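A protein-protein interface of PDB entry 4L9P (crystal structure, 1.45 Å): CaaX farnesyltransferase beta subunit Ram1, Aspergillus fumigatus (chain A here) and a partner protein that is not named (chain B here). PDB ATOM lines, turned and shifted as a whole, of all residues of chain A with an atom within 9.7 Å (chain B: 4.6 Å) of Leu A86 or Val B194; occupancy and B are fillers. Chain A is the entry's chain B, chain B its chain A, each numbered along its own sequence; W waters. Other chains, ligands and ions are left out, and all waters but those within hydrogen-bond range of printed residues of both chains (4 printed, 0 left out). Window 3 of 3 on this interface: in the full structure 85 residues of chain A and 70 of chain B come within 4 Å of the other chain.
Of the printed residues of chain B, Leu A86 touches Val B194, Arg B195 and Glu B254.
Of chain A, only Leu A86 (3.8 Å) comes within 4 Å of Val B194.
No residue of chain A comes within 4 Å of Leu B190.
Printed residues of chain A within 4 Å of Asn B258: Asp A84 and Asn A361.
Printed residues of chain B within 4 Å of Thr A88: Asp B193 (2.7 Å) and Arg B195 (3.0 Å).
Printed residues of chain A within 4 Å of Asp B193: Thr A88, Glu A89 and Thr A90.
Of the printed residues of chain B, Thr A90 touches Asp B193 and Arg B195.
Glu A92 touches none of the printed residues of chain B.
Asn B196 touches none of the printed residues of chain A.
The nearest residue of chain B that does not touch Leu A86 is Ala B255 (4.2 Å).
Of the 13 printed residues of chain A, 7 touch a printed residue of chain B.
Printed residues of chain B that touch a printed residue of chain A: Asp B193, Val B194, Arg B195, Glu B254, Ala B255 and Asn B258.
Hydrophobic or aromatic side chains of chain B that line the printed part of chain A: Val B194 and Ala B255.
Among the printed residues, Asp or Glu carboxylates within 4 Å of a Lys or Arg side-chain nitrogen of the other chain: Asp A84 with Arg B195 (3.1 Å).
The side-chain carboxylate (OD1) of Asp B193 sits close to the backbone NH (N) of Arg B195 (3.0 Å).
O of Val B194 is in hydrogen-bond range of NE1 of Trp B200 (2.9 Å).
O of Val B194 lies within hydrogen-bond range of ND2 of Asn B258, 3.0 Å away.
The guanidinium group (NH2) of Arg B251 is in salt-bridge range of the side-chain carboxylate (OE2) of Glu B254 (2.8 Å).
N of Thr A88 lies within hydrogen-bond range of OG1 of Thr A91.
O of Thr A91 is in hydrogen-bond range of OG of Ser A95, at 3.2 Å.
OD1 of Asp B193 lies within hydrogen-bond range of OG1 of Thr A88.
The side-chain carboxylate (OD2) of Asp B193 sits at hydrogen-bond distance from the side-chain hydroxyl (OG1) of Thr A90 (2.7 Å).
NH2 of Arg B195 lies within salt-bridge range of OD2 of Asp A84.
NH2 of Arg B195 sits at hydrogen-bond distance from O of Leu A86, 2.9 Å away.
The side-chain hydroxyl (OG1) of Thr A88 sits at hydrogen-bond distance from the guanidinium group (NH1) of Arg B195.
ND2 of Asn A361 is in hydrogen-bond range of O of Arg B195 (3.3 Å).
The side-chain amide oxygen (OD1) of Asn B258 is in hydrogen-bond range of the side-chain amide nitrogen (ND2) of Asn A361 (2.9 Å).
CB of Ala B255 touches OD2 of Asp A84, at 3.3 Å.
OD2 of Asp A84 touches N of Asn B258 (3.7 Å).
Leu A86 touches Val B194 (CD2 to CG1, 3.8 Å).
Leu A86 touches Glu B254.
Glu A89 touches Asp B193 (N to OD2, 3.7 Å).
Arg B195 touches Thr A90.
Thr A91 touches Arg B195.
Water W1 lies within hydrogen-bond range of O of Ala B192 (2.8 Å) and N of Glu A89 (2.9 Å).
Water W2 bridges O of Thr A360 (2.8 Å) and O of Arg B195 (3.4 Å).
Water W3 bridges the side-chain carboxylate (OD2) of Asp B193 (2.8 Å) and the side-chain carboxylate (OE1) of Glu A89 (3.5 Å).
Water W4 lies within hydrogen-bond range of the backbone carbonyl oxygen (O) of Glu B254, the backbone NH (N) of Leu A86 and the backbone NH (N) of Leu A85.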
ATOM      1  N   HIS A  83      -1.266  22.975 -28.686  1.00  0.00           N
ATOM      2  CA  HIS A  83      -2.077  22.674 -27.501  1.00  0.00           C
ATOM      3  C   HIS A  83      -3.349  21.947 -27.891  1.00  0.00           C
ATOM      4  O   HIS A  83      -4.193  22.461 -28.624  1.00  0.00           O
ATOM      5  CB  HIS A  83      -2.410  23.932 -26.682  1.00  0.00           C
ATOM      6  CG  HIS A  83      -1.389  24.272 -25.627  1.00  0.00           C
ATOM      7  ND1 HIS A  83      -0.319  25.112 -25.859  1.00  0.00           N
ATOM      8  CD2 HIS A  83      -1.293  23.901 -24.326  1.00  0.00           C
ATOM      9  CE1 HIS A  83       0.391  25.239 -24.756  1.00  0.00           C
ATOM     10  NE2 HIS A  83      -0.186  24.530 -23.807  1.00  0.00           N
ATOM     11  N   ASP A  84      -3.459  20.736 -27.371  1.00  0.00           N
ATOM     12  CA  ASP A  84      -4.595  19.846 -27.587  1.00  0.00           C
ATOM     13  C   ASP A  84      -5.842  20.472 -26.975  1.00  0.00           C
ATOM     14  O   ASP A  84      -5.771  21.134 -25.960  1.00  0.00           O
ATOM     15  CB  ASP A  84      -4.402  18.546 -26.803  1.00  0.00           C
ATOM     16  CG  ASP A  84      -3.342  17.560 -27.401  1.00  0.00           C
ATOM     17  OD1 ASP A  84      -3.003  17.622 -28.579  1.00  0.00           O
ATOM     18  OD2 ASP A  84      -2.892  16.657 -26.638  1.00  0.00           O
ATOM     19  N   LEU A  85      -7.008  20.209 -27.544  1.00  0.00           N
ATOM     20  CA  LEU A  85      -8.224  20.745 -26.947  1.00  0.00           C
ATOM     21  C   LEU A  85      -8.674  20.016 -25.703  1.00  0.00           C
ATOM     22  O   LEU A  85      -9.291  20.587 -24.809  1.00  0.00           O
ATOM     23  CB  LEU A  85      -9.372  20.649 -27.937  1.00  0.00           C
ATOM     24  CG  LEU A  85      -9.096  21.307 -29.270  1.00  0.00           C
ATOM     25  CD1 LEU A  85     -10.341  21.118 -30.173  1.00  0.00           C
ATOM     26  CD2 LEU A  85      -8.779  22.807 -29.100  1.00  0.00           C
ATOM     27  N   LEU A  86      -8.369  18.729 -25.634  1.00  0.00           N
ATOM     28  CA  LEU A  86      -8.874  17.919 -24.519  1.00  0.00           C
ATOM     29  C   LEU A  86      -8.179  18.261 -23.204  1.00  0.00           C
ATOM     30  O   LEU A  86      -6.944  18.174 -23.124  1.00  0.00           O
ATOM     31  CB  LEU A  86      -8.622  16.458 -24.846  1.00  0.00           C
ATOM     32  CG  LEU A  86      -8.994  15.482 -23.718  1.00  0.00           C
ATOM     33  CD1 LEU A  86     -10.518  15.407 -23.491  1.00  0.00           C
ATOM     34  CD2 LEU A  86      -8.404  14.088 -23.997  1.00  0.00           C
ATOM     35  N   SER A  87      -8.955  18.570 -22.170  1.00  0.00           N
ATOM     36  CA  SER A  87      -8.429  18.815 -20.825  1.00  0.00           C
ATOM     37  C   SER A  87      -8.552  17.540 -19.977  1.00  0.00           C
ATOM     38  O   SER A  87      -9.643  16.926 -19.913  1.00  0.00           O
ATOM     39  CB  SER A  87      -9.258  19.906 -20.152  1.00  0.00           C
ATOM     40  OG  SER A  87      -8.753  20.156 -18.854  1.00  0.00           O
ATOM     41  N   THR A  88      -7.437  17.109 -19.359  1.00  0.00           N
ATOM     42  CA  THR A  88      -7.466  16.062 -18.348  1.00  0.00           C
ATOM     43  C   THR A  88      -6.658  16.500 -17.132  1.00  0.00           C
ATOM     44  O   THR A  88      -6.054  17.591 -17.152  1.00  0.00           O
ATOM     45  CB  THR A  88      -6.856  14.750 -18.862  1.00  0.00           C
ATOM     46  OG1 THR A  88      -5.479  14.960 -19.205  1.00  0.00           O
ATOM     47  CG2 THR A  88      -7.631  14.169 -20.073  1.00  0.00           C
ATOM     48  N   GLU A  89      -6.616  15.708 -16.065  1.00  0.00           N
ATOM     49  CA  GLU A  89      -5.898  16.137 -14.887  1.00  0.00           C
ATOM     50  C   GLU A  89      -4.430  16.430 -15.214  1.00  0.00           C
ATOM     51  O   GLU A  89      -3.851  17.371 -14.686  1.00  0.00           O
ATOM     52  CB  GLU A  89      -5.985  15.063 -13.801  1.00  0.00           C
ATOM     53  CG  GLU A  89      -5.203  15.411 -12.546  1.00  0.00           C
ATOM     54  CD  GLU A  89      -5.339  14.397 -11.414  1.00  0.00           C
ATOM     55  OE1 GLU A  89      -4.979  13.194 -11.568  1.00  0.00           O
ATOM     56  OE2 GLU A  89      -5.810  14.811 -10.333  1.00  0.00           O
ATOM     57  N   THR A  90      -3.852  15.640 -16.113  1.00  0.00           N
ATOM     58  CA  THR A  90      -2.455  15.875 -16.519  1.00  0.00           C
ATOM     59  C   THR A  90      -2.284  17.282 -17.081  1.00  0.00           C
ATOM     60  O   THR A  90      -1.323  17.970 -16.701  1.00  0.00           O
ATOM     61  CB  THR A  90      -2.008  14.823 -17.614  1.00  0.00           C
ATOM     62  OG1 THR A  90      -1.981  13.536 -16.997  1.00  0.00           O
ATOM     63  CG2 THR A  90      -0.630  15.118 -18.173  1.00  0.00           C
ATOM     64  N   THR A  91      -3.177  17.713 -17.994  1.00  0.00           N
ATOM     65  CA  THR A  91      -2.988  19.037 -18.576  1.00  0.00           C
ATOM     66  C   THR A  91      -3.328  20.116 -17.596  1.00  0.00           C
ATOM     67  O   THR A  91      -2.726  21.203 -17.698  1.00  0.00           O
ATOM     68  CB  THR A  91      -3.734  19.234 -19.886  1.00  0.00           C
ATOM     69  OG1 THR A  91      -5.129  19.006 -19.673  1.00  0.00           O
ATOM     70  CG2 THR A  91      -3.189  18.257 -20.938  1.00  0.00           C
ATOM     71  N   GLU A  92      -4.237  19.881 -16.654  1.00  0.00           N
ATOM     72  CA  GLU A  92      -4.532  20.910 -15.645  1.00  0.00           C
ATOM     73  C   GLU A  92      -3.305  21.166 -14.800  1.00  0.00           C
ATOM     74  O   GLU A  92      -2.932  22.329 -14.557  1.00  0.00           O
ATOM     75  CB  GLU A  92      -5.661  20.445 -14.739  1.00  0.00           C
ATOM     76  CG  GLU A  92      -7.000  20.391 -15.383  1.00  0.00           C
ATOM     77  CD  GLU A  92      -8.011  19.787 -14.387  1.00  0.00           C
ATOM     78  OE1 GLU A  92      -8.177  20.380 -13.287  1.00  0.00           O
ATOM     79  OE2 GLU A  92      -8.583  18.701 -14.653  1.00  0.00           O
ATOM     80  N   SER A  95      -0.502  22.895 -16.953  1.00  0.00           N
ATOM     81  CA  SER A  95      -0.824  24.298 -17.179  1.00  0.00           C
ATOM     82  C   SER A  95      -0.636  25.128 -15.938  1.00  0.00           C
ATOM     83  O   SER A  95      -0.080  26.233 -15.999  1.00  0.00           O
ATOM     84  CB  SER A  95      -2.265  24.390 -17.659  1.00  0.00           C
ATOM     85  OG  SER A  95      -2.278  24.029 -19.019  1.00  0.00           O
ATOM     86  N   THR A 360       7.322  10.411 -18.171  1.00  0.00           N
ATOM     87  CA  THR A 360       6.474  10.962 -19.217  1.00  0.00           C
ATOM     88  C   THR A 360       5.141  11.465 -18.664  1.00  0.00           C
ATOM     89  O   THR A 360       4.455  10.778 -17.895  1.00  0.00           O
ATOM     90  CB  THR A 360       6.210   9.880 -20.272  1.00  0.00           C
ATOM     91  OG1 THR A 360       7.509   9.479 -20.757  1.00  0.00           O
ATOM     92  CG2 THR A 360       5.303  10.372 -21.434  1.00  0.00           C
ATOM     93  N   ASN A 361       4.770  12.678 -19.119  1.00  0.00           N
ATOM     94  CA  ASN A 361       3.500  13.300 -18.737  1.00  0.00           C
ATOM     95  C   ASN A 361       3.364  13.648 -17.248  1.00  0.00           C
ATOM     96  O   ASN A 361       2.259  13.880 -16.767  1.00  0.00           O
ATOM     97  CB  ASN A 361       2.307  12.483 -19.245  1.00  0.00           C
ATOM     98  CG  ASN A 361       1.915  12.865 -20.665  1.00  0.00           C
ATOM     99  OD1 ASN A 361       1.919  14.067 -21.009  1.00  0.00           O
ATOM    100  ND2 ASN A 361       1.525  11.899 -21.472  1.00  0.00           N
ATOM    101  N   LEU B 190      -7.346   5.194 -18.596  1.00  0.00           N
ATOM    102  CA  LEU B 190      -7.036   5.967 -19.825  1.00  0.00           C
ATOM    103  C   LEU B 190      -8.247   6.724 -20.361  1.00  0.00           C
ATOM    104  O   LEU B 190      -8.117   7.720 -21.049  1.00  0.00           O
ATOM    105  CB  LEU B 190      -6.416   5.064 -20.875  1.00  0.00           C
ATOM    106  CG  LEU B 190      -5.040   4.532 -20.500  1.00  0.00           C
ATOM    107  CD1 LEU B 190      -4.579   3.612 -21.609  1.00  0.00           C
ATOM    108  CD2 LEU B 190      -4.049   5.713 -20.284  1.00  0.00           C
ATOM    109  N   ALA B 192     -10.338   8.187 -18.207  1.00  0.00           N
ATOM    110  CA  ALA B 192     -10.338   9.355 -17.320  1.00  0.00           C
ATOM    111  C   ALA B 192      -9.202  10.303 -17.713  1.00  0.00           C
ATOM    112  O   ALA B 192      -9.402  11.526 -17.639  1.00  0.00           O
ATOM    113  CB  ALA B 192     -10.158   8.889 -15.863  1.00  0.00           C
ATOM    114  N   ASP B 193      -8.038   9.764 -18.061  1.00  0.00           N
ATOM    115  CA  ASP B 193      -6.901  10.655 -18.429  1.00  0.00           C
ATOM    116  C   ASP B 193      -6.037   9.881 -19.425  1.00  0.00           C
ATOM    117  O   ASP B 193      -5.204   9.056 -19.030  1.00  0.00           O
ATOM    118  CB  ASP B 193      -6.090  11.092 -17.206  1.00  0.00           C
ATOM    119  CG  ASP B 193      -5.044  12.123 -17.540  1.00  0.00           C
ATOM    120  OD1 ASP B 193      -4.809  12.344 -18.750  1.00  0.00           O
ATOM    121  OD2 ASP B 193      -4.481  12.679 -16.577  1.00  0.00           O
ATOM    122  N   VAL B 194      -6.232  10.130 -20.718  1.00  0.00           N
ATOM    123  CA  VAL B 194      -5.498   9.424 -21.761  1.00  0.00           C
ATOM    124  C   VAL B 194      -3.982   9.700 -21.684  1.00  0.00           C
ATOM    125  O   VAL B 194      -3.188   8.963 -22.296  1.00  0.00           O
ATOM    126  CB  VAL B 194      -6.098   9.777 -23.163  1.00  0.00           C
ATOM    127  CG1 VAL B 194      -5.841  11.283 -23.528  1.00  0.00           C
ATOM    128  CG2 VAL B 194      -5.588   8.810 -24.234  1.00  0.00           C
ATOM    129  N   ARG B 195      -3.608  10.705 -20.907  1.00  0.00           N
ATOM    130  CA  ARG B 195      -2.176  11.025 -20.726  1.00  0.00           C
ATOM    131  C   ARG B 195      -1.525  10.326 -19.555  1.00  0.00           C
ATOM    132  O   ARG B 195      -0.404  10.658 -19.159  1.00  0.00           O
ATOM    133  CB  ARG B 195      -1.989  12.547 -20.586  1.00  0.00           C
ATOM    134  CG  ARG B 195      -2.436  13.222 -21.896  1.00  0.00           C
ATOM    135  CD  ARG B 195      -2.897  14.574 -21.617  1.00  0.00           C
ATOM    136  NE  ARG B 195      -3.237  15.351 -22.831  1.00  0.00           N
ATOM    137  CZ  ARG B 195      -4.391  15.994 -22.972  1.00  0.00           C
ATOM    138  NH1 ARG B 195      -5.331  15.910 -22.045  1.00  0.00           N
ATOM    139  NH2 ARG B 195      -4.581  16.758 -24.044  1.00  0.00           N
ATOM    140  N   ASN B 196      -2.245   9.347 -18.956  1.00  0.00           N
ATOM    141  CA  ASN B 196      -1.666   8.622 -17.813  1.00  0.00           C
ATOM    142  C   ASN B 196      -0.643   7.598 -18.259  1.00  0.00           C
ATOM    143  O   ASN B 196      -0.971   6.490 -18.633  1.00  0.00           O
ATOM    144  CB  ASN B 196      -2.765   7.966 -16.976  1.00  0.00           C
ATOM    145  CG  ASN B 196      -2.230   7.318 -15.737  1.00  0.00           C
ATOM    146  OD1 ASN B 196      -1.030   7.071 -15.627  1.00  0.00           O
ATOM    147  ND2 ASN B 196      -3.110   6.997 -14.806  1.00  0.00           N
ATOM    148  N   TRP B 200      -0.393   3.393 -19.498  1.00  0.00           N
ATOM    149  CA  TRP B 200       0.199   2.899 -20.741  1.00  0.00           C
ATOM    150  C   TRP B 200       1.317   1.904 -20.454  1.00  0.00           C
ATOM    151  O   TRP B 200       1.421   0.888 -21.145  1.00  0.00           O
ATOM    152  CB  TRP B 200       0.748   4.060 -21.586  1.00  0.00           C
ATOM    153  CG  TRP B 200      -0.333   4.832 -22.263  1.00  0.00           C
ATOM    154  CD1 TRP B 200      -0.862   6.048 -21.857  1.00  0.00           C
ATOM    155  CD2 TRP B 200      -1.025   4.462 -23.475  1.00  0.00           C
ATOM    156  NE1 TRP B 200      -1.834   6.454 -22.764  1.00  0.00           N
ATOM    157  CE2 TRP B 200      -1.964   5.491 -23.750  1.00  0.00           C
ATOM    158  CE3 TRP B 200      -0.955   3.346 -24.329  1.00  0.00           C
ATOM    159  CZ2 TRP B 200      -2.835   5.445 -24.864  1.00  0.00           C
ATOM    160  CZ3 TRP B 200      -1.821   3.313 -25.453  1.00  0.00           C
ATOM    161  CH2 TRP B 200      -2.713   4.369 -25.716  1.00  0.00           C
ATOM    162  N   ARG B 251      -6.517   6.497 -29.634  1.00  0.00           N
ATOM    163  CA  ARG B 251      -6.230   7.357 -28.502  1.00  0.00           C
ATOM    164  C   ARG B 251      -5.469   8.618 -28.925  1.00  0.00           C
ATOM    165  O   ARG B 251      -5.730   9.697 -28.402  1.00  0.00           O
ATOM    166  CB  ARG B 251      -5.431   6.600 -27.436  1.00  0.00           C
ATOM    167  CG  ARG B 251      -6.150   5.377 -26.845  1.00  0.00           C
ATOM    168  CD  ARG B 251      -7.401   5.711 -25.980  1.00  0.00           C
ATOM    169  NE  ARG B 251      -8.549   6.147 -26.672  1.00  0.00           N
ATOM    170  CZ  ARG B 251      -9.358   5.335 -27.378  1.00  0.00           C
ATOM    171  NH1 ARG B 251      -9.042   4.048 -27.518  1.00  0.00           N
ATOM    172  NH2 ARG B 251     -10.460   5.814 -27.992  1.00  0.00           N
ATOM    173  N   GLU B 254      -7.581  11.529 -30.043  1.00  0.00           N
ATOM    174  CA  GLU B 254      -8.229  12.316 -28.992  1.00  0.00           C
ATOM    175  C   GLU B 254      -7.365  13.444 -28.466  1.00  0.00           C
ATOM    176  O   GLU B 254      -7.898  14.411 -27.886  1.00  0.00           O
ATOM    177  CB  GLU B 254      -8.616  11.426 -27.802  1.00  0.00           C
ATOM    178  CG  GLU B 254      -9.587  10.319 -28.178  1.00  0.00           C
ATOM    179  CD  GLU B 254      -9.783   9.260 -27.100  1.00  0.00           C
ATOM    180  OE1 GLU B 254      -9.034   9.180 -26.122  1.00  0.00           O
ATOM    181  OE2 GLU B 254     -10.744   8.498 -27.235  1.00  0.00           O
ATOM    182  N   ALA B 255      -6.030  13.335 -28.643  1.00  0.00           N
ATOM    183  CA  ALA B 255      -5.080  14.303 -28.029  1.00  0.00           C
ATOM    184  C   ALA B 255      -3.734  14.064 -28.662  1.00  0.00           C
ATOM    185  O   ALA B 255      -2.895  13.367 -28.138  1.00  0.00           O
ATOM    186  CB  ALA B 255      -5.011  14.141 -26.475  1.00  0.00           C
ATOM    187  N   ASN B 258      -0.153  14.144 -27.001  1.00  0.00           N
ATOM    188  CA  ASN B 258       0.124  13.278 -25.840  1.00  0.00           C
ATOM    189  C   ASN B 258       1.219  12.271 -26.201  1.00  0.00           C
ATOM    190  O   ASN B 258       1.002  11.387 -27.034  1.00  0.00           O
ATOM    191  CB  ASN B 258      -1.170  12.562 -25.570  1.00  0.00           C
ATOM    192  CG  ASN B 258      -1.094  11.472 -24.524  1.00  0.00           C
ATOM    193  OD1 ASN B 258      -0.146  11.367 -23.741  1.00  0.00           O
ATOM    194  ND2 ASN B 258      -2.167  10.660 -24.488  1.00  0.00           N
HETATM  195  O   HOH W   1      -8.580  13.575 -15.978  1.00  0.00           O
HETATM  196  O   HOH W   2       1.983  10.347 -16.730  1.00  0.00           O
HETATM  197  O   HOH W   3      -4.232  11.135 -14.283  1.00  0.00           O
HETATM  198  O   HOH W   4      -7.248  17.136 -27.784  1.00  0.00           O
